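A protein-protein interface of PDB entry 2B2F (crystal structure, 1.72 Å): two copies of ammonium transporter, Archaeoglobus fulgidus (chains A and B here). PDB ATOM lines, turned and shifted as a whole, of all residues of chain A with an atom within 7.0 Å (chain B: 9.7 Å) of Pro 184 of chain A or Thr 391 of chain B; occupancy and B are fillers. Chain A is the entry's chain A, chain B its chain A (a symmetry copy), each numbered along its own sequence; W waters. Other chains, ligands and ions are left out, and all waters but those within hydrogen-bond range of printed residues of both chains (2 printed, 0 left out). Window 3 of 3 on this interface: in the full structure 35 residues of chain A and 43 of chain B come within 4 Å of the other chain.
Ala 28 of chain A touches none of the printed residues of chain B. No residue of chain B comes within 4 Å of Glu 183 of chain A. Printed residues of chain B within 4 Å of Ser 186 of chain A: Ala 389 (3.4 Å) and Tyr 390 (3.6 Å). Printed residues of chain B within 4 Å of Ile 187 of chain A: Val 37, Glu 387, Val 388 and Ala 389. Printed residues of chain A within 4 Å of Val 37 of chain B: Ile 187. Of the printed residues of chain A, Ala 389 of chain B touches His 185, Ser 186 and Ile 187. Of chain A, only Pro 184 and His 185 come within 4 Å of Thr 391 of chain B.
O of Ala 28 of chain A sits close to ND1 of His 185 of chain A. O of Gly 29 of chain A sits at hydrogen-bond distance from N of His 185 of chain A. The backbone carbonyl oxygen (O) of Gly 29 of chain A is in hydrogen-bond range of the backbone NH (N) of Ser 186 of chain A (3.1 Å). O of Val 31 of chain A lies within hydrogen-bond range of ND1 of His 185 of chain A (2.9 Å). The backbone carbonyl oxygen (O) of Tyr 390 of chain B sits at hydrogen-bond distance from the guanidinium group (NH2) of Arg 33 of chain B (2.9 Å). N of Leu 382 of chain B lies within hydrogen-bond range of O of Glu 387 of chain B (3.3 Å).
Water W2 lies within hydrogen-bond range of O of Pro 184 of chain A (2.6 Å), O of Val 388 of chain B (2.7 Å) and OG1 of Thr 391 of chain B (3.0 Å). Water W1 bridges the backbone carbonyl oxygen of Thr 391 of chain B (2.7 Å) and the backbone NH of Arg 33 of chain A (2.8 Å).
Position printed for both chains: 33. Of the 11 pairs that touch across the chains among the printed residues, none has its exchanged pair printed and touching as well.
Hydrophobic or aromatic side chains of chain A within 4 Å of the printed part of chain B: His 185, Ile 187 and Leu 247. Along chain A the printed residues that touch a printed residue of chain B span positions 184 to 247. Of the 9 printed residues of chain B, 6 touch a printed residue of chain A. Printed residues of chain B that touch a printed residue of chain A: Val 37, Glu 387, Val 388, Ala 389, Tyr 390 and Thr 391. Hydrophobic or aromatic side chains of chain B within 4 Å of the printed part of chain A: Val 37 and Tyr 390. Among the printed residues, 11 pairs touch across the chains.
Among the printed residues, pairs that only touch across the chains: Pro 184 of chain A with Thr 391 of chain B (3.8 Å), His 185 of chain A with Ala 389 of chain B (3.8 Å), His 185 of chain A with Tyr 390 of chain B (3.2 Å), Ser 186 of chain A with Ala 389 of chain B (3.4 Å), Ser 186 of chain A with Tyr 390 of chain B (3.6 Å), Ile 187 of chain A with Val 37 of chain B (3.9 Å), Ile 187 of chain A with Glu 387 of chain B (3.8 Å) and Ile 187 of chain A with Val 388 of chain B (3.5 Å).
The backbone carbonyl oxygen (O) of His 185 of chain A lies within hydrogen-bond range of the backbone NH (N) of Thr 391 of chain B, at 3.0 Å. The backbone NH (N) of Ile 187 of chain A lies within hydrogen-bond range of the backbone carbonyl oxygen (O) of Ala 389 of chain B, 2.9 Å away. OE1 of Glu 387 of chain B sits at hydrogen-bond distance from N of Leu 247 of chain A, 3.1 Å away.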
ATOM      1  N   ALA A  28      17.129   3.942 -20.341  1.00  0.00           N
ATOM      2  CA  ALA A  28      16.850   4.427 -21.691  1.00  0.00           C
ATOM      3  C   ALA A  28      15.640   5.352 -21.801  1.00  0.00           C
ATOM      4  O   ALA A  28      15.670   6.346 -22.532  1.00  0.00           O
ATOM      5  CB  ALA A  28      16.685   3.252 -22.635  1.00  0.00           C
ATOM      6  N   GLY A  29      14.575   5.038 -21.079  1.00  0.00           N
ATOM      7  CA  GLY A  29      13.392   5.871 -21.172  1.00  0.00           C
ATOM      8  C   GLY A  29      13.634   7.272 -20.659  1.00  0.00           C
ATOM      9  O   GLY A  29      12.960   8.213 -21.075  1.00  0.00           O
ATOM     10  N   MET A  30      14.607   7.418 -19.766  1.00  0.00           N
ATOM     11  CA  MET A  30      14.899   8.716 -19.181  1.00  0.00           C
ATOM     12  C   MET A  30      15.863   9.603 -19.956  1.00  0.00           C
ATOM     13  O   MET A  30      16.036  10.770 -19.609  1.00  0.00           O
ATOM     14  CB  MET A  30      15.398   8.528 -17.751  1.00  0.00           C
ATOM     15  CG  MET A  30      14.358   7.862 -16.873  1.00  0.00           C
ATOM     16  SD  MET A  30      14.818   7.738 -15.127  1.00  0.00           S
ATOM     17  CE  MET A  30      16.221   6.690 -15.252  1.00  0.00           C
ATOM     18  N   VAL A  31      16.496   9.071 -20.995  1.00  0.00           N
ATOM     19  CA  VAL A  31      17.406   9.892 -21.785  1.00  0.00           C
ATOM     20  C   VAL A  31      16.694  10.313 -23.068  1.00  0.00           C
ATOM     21  O   VAL A  31      15.566   9.892 -23.334  1.00  0.00           O
ATOM     22  CB  VAL A  31      18.714   9.138 -22.158  1.00  0.00           C
ATOM     23  CG1 VAL A  31      19.407   8.632 -20.899  1.00  0.00           C
ATOM     24  CG2 VAL A  31      18.417   7.997 -23.117  1.00  0.00           C
ATOM     25  N   ARG A  32      17.355  11.141 -23.866  1.00  0.00           N
ATOM     26  CA  ARG A  32      16.773  11.613 -25.110  1.00  0.00           C
ATOM     27  C   ARG A  32      16.713  10.538 -26.173  1.00  0.00           C
ATOM     28  O   ARG A  32      17.499   9.587 -26.170  1.00  0.00           O
ATOM     29  CB  ARG A  32      17.562  12.807 -25.627  1.00  0.00           C
ATOM     30  CG  ARG A  32      17.211  14.097 -24.909  1.00  0.00           C
ATOM     31  CD  ARG A  32      18.276  15.153 -25.127  1.00  0.00           C
ATOM     32  NE  ARG A  32      19.517  14.810 -24.435  1.00  0.00           N
ATOM     33  CZ  ARG A  32      20.535  15.649 -24.272  1.00  0.00           C
ATOM     34  NH1 ARG A  32      20.461  16.882 -24.758  1.00  0.00           N
ATOM     35  NH2 ARG A  32      21.617  15.265 -23.606  1.00  0.00           N
ATOM     36  N   ARG A  33      15.772  10.707 -27.088  1.00  0.00           N
ATOM     37  CA  ARG A  33      15.560   9.767 -28.169  1.00  0.00           C
ATOM     38  C   ARG A  33      16.849   9.414 -28.906  1.00  0.00           C
ATOM     39  O   ARG A  33      17.064   8.251 -29.264  1.00  0.00           O
ATOM     40  CB  ARG A  33      14.532  10.361 -29.129  1.00  0.00           C
ATOM     41  CG  ARG A  33      14.207   9.509 -30.332  1.00  0.00           C
ATOM     42  CD  ARG A  33      13.132  10.166 -31.206  1.00  0.00           C
ATOM     43  NE  ARG A  33      13.061   9.519 -32.519  1.00  0.00           N
ATOM     44  CZ  ARG A  33      12.186   9.829 -33.472  1.00  0.00           C
ATOM     45  NH1 ARG A  33      11.288  10.785 -33.269  1.00  0.00           N
ATOM     46  NH2 ARG A  33      12.215   9.179 -34.629  1.00  0.00           N
ATOM     47  N   ILE A 182      16.692  17.953 -19.287  1.00  0.00           N
ATOM     48  CA  ILE A 182      16.764  16.935 -20.317  1.00  0.00           C
ATOM     49  C   ILE A 182      15.484  16.155 -20.069  1.00  0.00           C
ATOM     50  O   ILE A 182      15.289  15.623 -18.976  1.00  0.00           O
ATOM     51  CB  ILE A 182      17.960  16.001 -20.100  1.00  0.00           C
ATOM     52  CG1 ILE A 182      19.257  16.813 -20.047  1.00  0.00           C
ATOM     53  CG2 ILE A 182      17.995  14.953 -21.188  1.00  0.00           C
ATOM     54  CD1 ILE A 182      19.491  17.687 -21.246  1.00  0.00           C
ATOM     55  N   GLU A 183      14.604  16.089 -21.058  1.00  0.00           N
ATOM     56  CA  GLU A 183      13.348  15.368 -20.870  1.00  0.00           C
ATOM     57  C   GLU A 183      13.427  13.883 -21.233  1.00  0.00           C
ATOM     58  O   GLU A 183      14.098  13.496 -22.191  1.00  0.00           O
ATOM     59  CB  GLU A 183      12.230  16.011 -21.696  1.00  0.00           C
ATOM     60  CG  GLU A 183      11.976  17.490 -21.416  1.00  0.00           C
ATOM     61  CD  GLU A 183      11.694  17.771 -19.952  1.00  0.00           C
ATOM     62  OE1 GLU A 183      10.984  16.959 -19.318  1.00  0.00           O
ATOM     63  OE2 GLU A 183      12.174  18.809 -19.440  1.00  0.00           O
ATOM     64  N   PRO A 184      12.744  13.028 -20.460  1.00  0.00           N
ATOM     65  CA  PRO A 184      12.758  11.589 -20.749  1.00  0.00           C
ATOM     66  C   PRO A 184      12.009  11.375 -22.068  1.00  0.00           C
ATOM     67  O   PRO A 184      10.884  11.850 -22.219  1.00  0.00           O
ATOM     68  CB  PRO A 184      12.016  10.992 -19.558  1.00  0.00           C
ATOM     69  CG  PRO A 184      11.067  12.089 -19.167  1.00  0.00           C
ATOM     70  CD  PRO A 184      11.932  13.326 -19.269  1.00  0.00           C
ATOM     71  N   HIS A 185      12.608  10.661 -23.016  1.00  0.00           N
ATOM     72  CA  HIS A 185      11.946  10.465 -24.299  1.00  0.00           C
ATOM     73  C   HIS A 185      10.803   9.456 -24.252  1.00  0.00           C
ATOM     74  O   HIS A 185       9.888   9.516 -25.069  1.00  0.00           O
ATOM     75  CB  HIS A 185      12.959  10.051 -25.375  1.00  0.00           C
ATOM     76  CG  HIS A 185      13.170   8.570 -25.477  1.00  0.00           C
ATOM     77  ND1 HIS A 185      13.993   7.868 -24.624  1.00  0.00           N
ATOM     78  CD2 HIS A 185      12.634   7.653 -26.320  1.00  0.00           C
ATOM     79  CE1 HIS A 185      13.955   6.583 -24.933  1.00  0.00           C
ATOM     80  NE2 HIS A 185      13.137   6.426 -25.959  1.00  0.00           N
ATOM     81  N   SER A 186      10.847   8.527 -23.303  1.00  0.00           N
ATOM     82  CA  SER A 186       9.793   7.527 -23.212  1.00  0.00           C
ATOM     83  C   SER A 186       9.633   7.017 -21.798  1.00  0.00           C
ATOM     84  O   SER A 186      10.317   6.079 -21.376  1.00  0.00           O
ATOM     85  CB  SER A 186      10.085   6.345 -24.138  1.00  0.00           C
ATOM     86  OG  SER A 186       9.051   5.380 -24.026  1.00  0.00           O
ATOM     87  N   ILE A 187       8.732   7.640 -21.053  1.00  0.00           N
ATOM     88  CA  ILE A 187       8.520   7.200 -19.693  1.00  0.00           C
ATOM     89  C   ILE A 187       7.989   5.764 -19.691  1.00  0.00           C
ATOM     90  O   ILE A 187       8.357   4.964 -18.828  1.00  0.00           O
ATOM     91  CB  ILE A 187       7.570   8.171 -18.946  1.00  0.00           C
ATOM     92  CG1 ILE A 187       8.304   9.507 -18.727  1.00  0.00           C
ATOM     93  CG2 ILE A 187       7.132   7.576 -17.608  1.00  0.00           C
ATOM     94  CD1 ILE A 187       7.498  10.566 -17.979  1.00  0.00           C
ATOM     95  N   THR A 190      10.702   3.347 -19.610  1.00  0.00           N
ATOM     96  CA  THR A 190      11.303   3.299 -18.290  1.00  0.00           C
ATOM     97  C   THR A 190      10.448   2.460 -17.339  1.00  0.00           C
ATOM     98  O   THR A 190      10.982   1.686 -16.537  1.00  0.00           O
ATOM     99  CB  THR A 190      11.469   4.711 -17.718  1.00  0.00           C
ATOM    100  OG1 THR A 190      12.573   5.345 -18.370  1.00  0.00           O
ATOM    101  CG2 THR A 190      11.737   4.666 -16.227  1.00  0.00           C
ATOM    102  N   LEU A 247       7.709   8.527 -12.371  1.00  0.00           N
ATOM    103  CA  LEU A 247       9.145   8.332 -12.231  1.00  0.00           C
ATOM    104  C   LEU A 247       9.543   8.383 -10.760  1.00  0.00           C
ATOM    105  O   LEU A 247      10.375   7.590 -10.300  1.00  0.00           O
ATOM    106  CB  LEU A 247       9.903   9.397 -13.029  1.00  0.00           C
ATOM    107  CG  LEU A 247       9.692   9.324 -14.548  1.00  0.00           C
ATOM    108  CD1 LEU A 247      10.495  10.422 -15.241  1.00  0.00           C
ATOM    109  CD2 LEU A 247      10.122   7.959 -15.069  1.00  0.00           C
ATOM    110  N   ARG B  33      -2.181   8.814 -26.086  1.00  0.00           N
ATOM    111  CA  ARG B  33      -0.830   9.155 -25.694  1.00  0.00           C
ATOM    112  C   ARG B  33      -0.779  10.037 -24.450  1.00  0.00           C
ATOM    113  O   ARG B  33       0.078   9.844 -23.583  1.00  0.00           O
ATOM    114  CB  ARG B  33      -0.144   9.841 -26.874  1.00  0.00           C
ATOM    115  CG  ARG B  33       1.278  10.280 -26.625  1.00  0.00           C
ATOM    116  CD  ARG B  33       1.894  10.911 -27.879  1.00  0.00           C
ATOM    117  NE  ARG B  33       3.128  11.628 -27.550  1.00  0.00           N
ATOM    118  CZ  ARG B  33       3.919  12.226 -28.436  1.00  0.00           C
ATOM    119  NH1 ARG B  33       3.614  12.201 -29.728  1.00  0.00           N
ATOM    120  NH2 ARG B  33       5.015  12.853 -28.024  1.00  0.00           N
ATOM    121  N   VAL B  37       1.031   7.396 -19.365  1.00  0.00           N
ATOM    122  CA  VAL B  37       1.691   7.302 -18.070  1.00  0.00           C
ATOM    123  C   VAL B  37       0.691   7.010 -16.961  1.00  0.00           C
ATOM    124  O   VAL B  37       0.902   6.135 -16.123  1.00  0.00           O
ATOM    125  CB  VAL B  37       2.451   8.605 -17.741  1.00  0.00           C
ATOM    126  CG1 VAL B  37       2.954   8.576 -16.301  1.00  0.00           C
ATOM    127  CG2 VAL B  37       3.607   8.765 -18.700  1.00  0.00           C
ATOM    128  N   LEU B 382      -0.158  14.912 -17.789  1.00  0.00           N
ATOM    129  CA  LEU B 382       0.219  16.263 -17.418  1.00  0.00           C
ATOM    130  C   LEU B 382      -0.515  16.735 -16.179  1.00  0.00           C
ATOM    131  O   LEU B 382       0.102  17.150 -15.198  1.00  0.00           O
ATOM    132  CB  LEU B 382      -0.109  17.228 -18.546  1.00  0.00           C
ATOM    133  CG  LEU B 382       0.992  18.119 -19.133  1.00  0.00           C
ATOM    134  CD1 LEU B 382       2.300  18.011 -18.360  1.00  0.00           C
ATOM    135  CD2 LEU B 382       1.190  17.703 -20.573  1.00  0.00           C
ATOM    136  N   GLU B 386       1.989  15.544 -13.971  1.00  0.00           N
ATOM    137  CA  GLU B 386       2.896  16.566 -14.467  1.00  0.00           C
ATOM    138  C   GLU B 386       4.050  15.912 -15.222  1.00  0.00           C
ATOM    139  O   GLU B 386       5.220  16.249 -15.029  1.00  0.00           O
ATOM    140  CB  GLU B 386       3.432  17.412 -13.321  1.00  0.00           C
ATOM    141  CG  GLU B 386       2.357  18.245 -12.679  1.00  0.00           C
ATOM    142  CD  GLU B 386       2.910  19.300 -11.743  1.00  0.00           C
ATOM    143  OE1 GLU B 386       2.101  20.087 -11.204  1.00  0.00           O
ATOM    144  OE2 GLU B 386       4.147  19.344 -11.552  1.00  0.00           O
ATOM    145  N   GLU B 387       3.706  14.959 -16.079  1.00  0.00           N
ATOM    146  CA  GLU B 387       4.692  14.257 -16.884  1.00  0.00           C
ATOM    147  C   GLU B 387       4.171  14.163 -18.313  1.00  0.00           C
ATOM    148  O   GLU B 387       2.978  14.355 -18.563  1.00  0.00           O
ATOM    149  CB  GLU B 387       4.930  12.848 -16.327  1.00  0.00           C
ATOM    150  CG  GLU B 387       5.836  12.794 -15.106  1.00  0.00           C
ATOM    151  CD  GLU B 387       6.008  11.386 -14.548  1.00  0.00           C
ATOM    152  OE1 GLU B 387       7.033  11.140 -13.880  1.00  0.00           O
ATOM    153  OE2 GLU B 387       5.127  10.523 -14.754  1.00  0.00           O
ATOM    154  N   VAL B 388       5.078  13.878 -19.241  1.00  0.00           N
ATOM    155  CA  VAL B 388       4.750  13.713 -20.653  1.00  0.00           C
ATOM    156  C   VAL B 388       5.315  12.357 -21.050  1.00  0.00           C
ATOM    157  O   VAL B 388       6.511  12.117 -20.910  1.00  0.00           O
ATOM    158  CB  VAL B 388       5.392  14.816 -21.517  1.00  0.00           C
ATOM    159  CG1 VAL B 388       5.153  14.534 -22.995  1.00  0.00           C
ATOM    160  CG2 VAL B 388       4.793  16.168 -21.149  1.00  0.00           C
ATOM    161  N   ALA B 389       4.447  11.473 -21.532  1.00  0.00           N
ATOM    162  CA  ALA B 389       4.842  10.118 -21.917  1.00  0.00           C
ATOM    163  C   ALA B 389       6.017  10.037 -22.881  1.00  0.00           C
ATOM    164  O   ALA B 389       7.021   9.386 -22.603  1.00  0.00           O
ATOM    165  CB  ALA B 389       3.642   9.389 -22.504  1.00  0.00           C
ATOM    166  N   TYR B 390       5.889  10.700 -24.021  1.00  0.00           N
ATOM    167  CA  TYR B 390       6.946  10.664 -25.016  1.00  0.00           C
ATOM    168  C   TYR B 390       7.356  12.029 -25.506  1.00  0.00           C
ATOM    169  O   TYR B 390       6.554  12.955 -25.588  1.00  0.00           O
ATOM    170  CB  TYR B 390       6.514   9.852 -26.232  1.00  0.00           C
ATOM    171  CG  TYR B 390       5.801   8.570 -25.907  1.00  0.00           C
ATOM    172  CD1 TYR B 390       4.411   8.528 -25.811  1.00  0.00           C
ATOM    173  CD2 TYR B 390       6.515   7.386 -25.717  1.00  0.00           C
ATOM    174  CE1 TYR B 390       3.746   7.337 -25.533  1.00  0.00           C
ATOM    175  CE2 TYR B 390       5.859   6.187 -25.436  1.00  0.00           C
ATOM    176  CZ  TYR B 390       4.480   6.169 -25.350  1.00  0.00           C
ATOM    177  OH  TYR B 390       3.831   4.984 -25.090  1.00  0.00           O
ATOM    178  N   THR B 391       8.624  12.129 -25.854  1.00  0.00           N
ATOM    179  CA  THR B 391       9.194  13.350 -26.376  1.00  0.00           C
ATOM    180  C   THR B 391      10.049  12.883 -27.542  1.00  0.00           C
ATOM    181  O   THR B 391      11.263  12.671 -27.310  1.00  0.00           O
ATOM    182  CB  THR B 391      10.074  14.046 -25.327  1.00  0.00           C
ATOM    183  OG1 THR B 391       9.248  14.547 -24.267  1.00  0.00           O
ATOM    184  CG2 THR B 391      10.849  15.190 -25.963  1.00  0.00           C
HETATM  185  O   HOH W   1      13.939  12.817 -27.052  1.00  0.00           O
HETATM  186  O   HOH W   2       8.795  13.325 -21.620  1.00  0.00           O
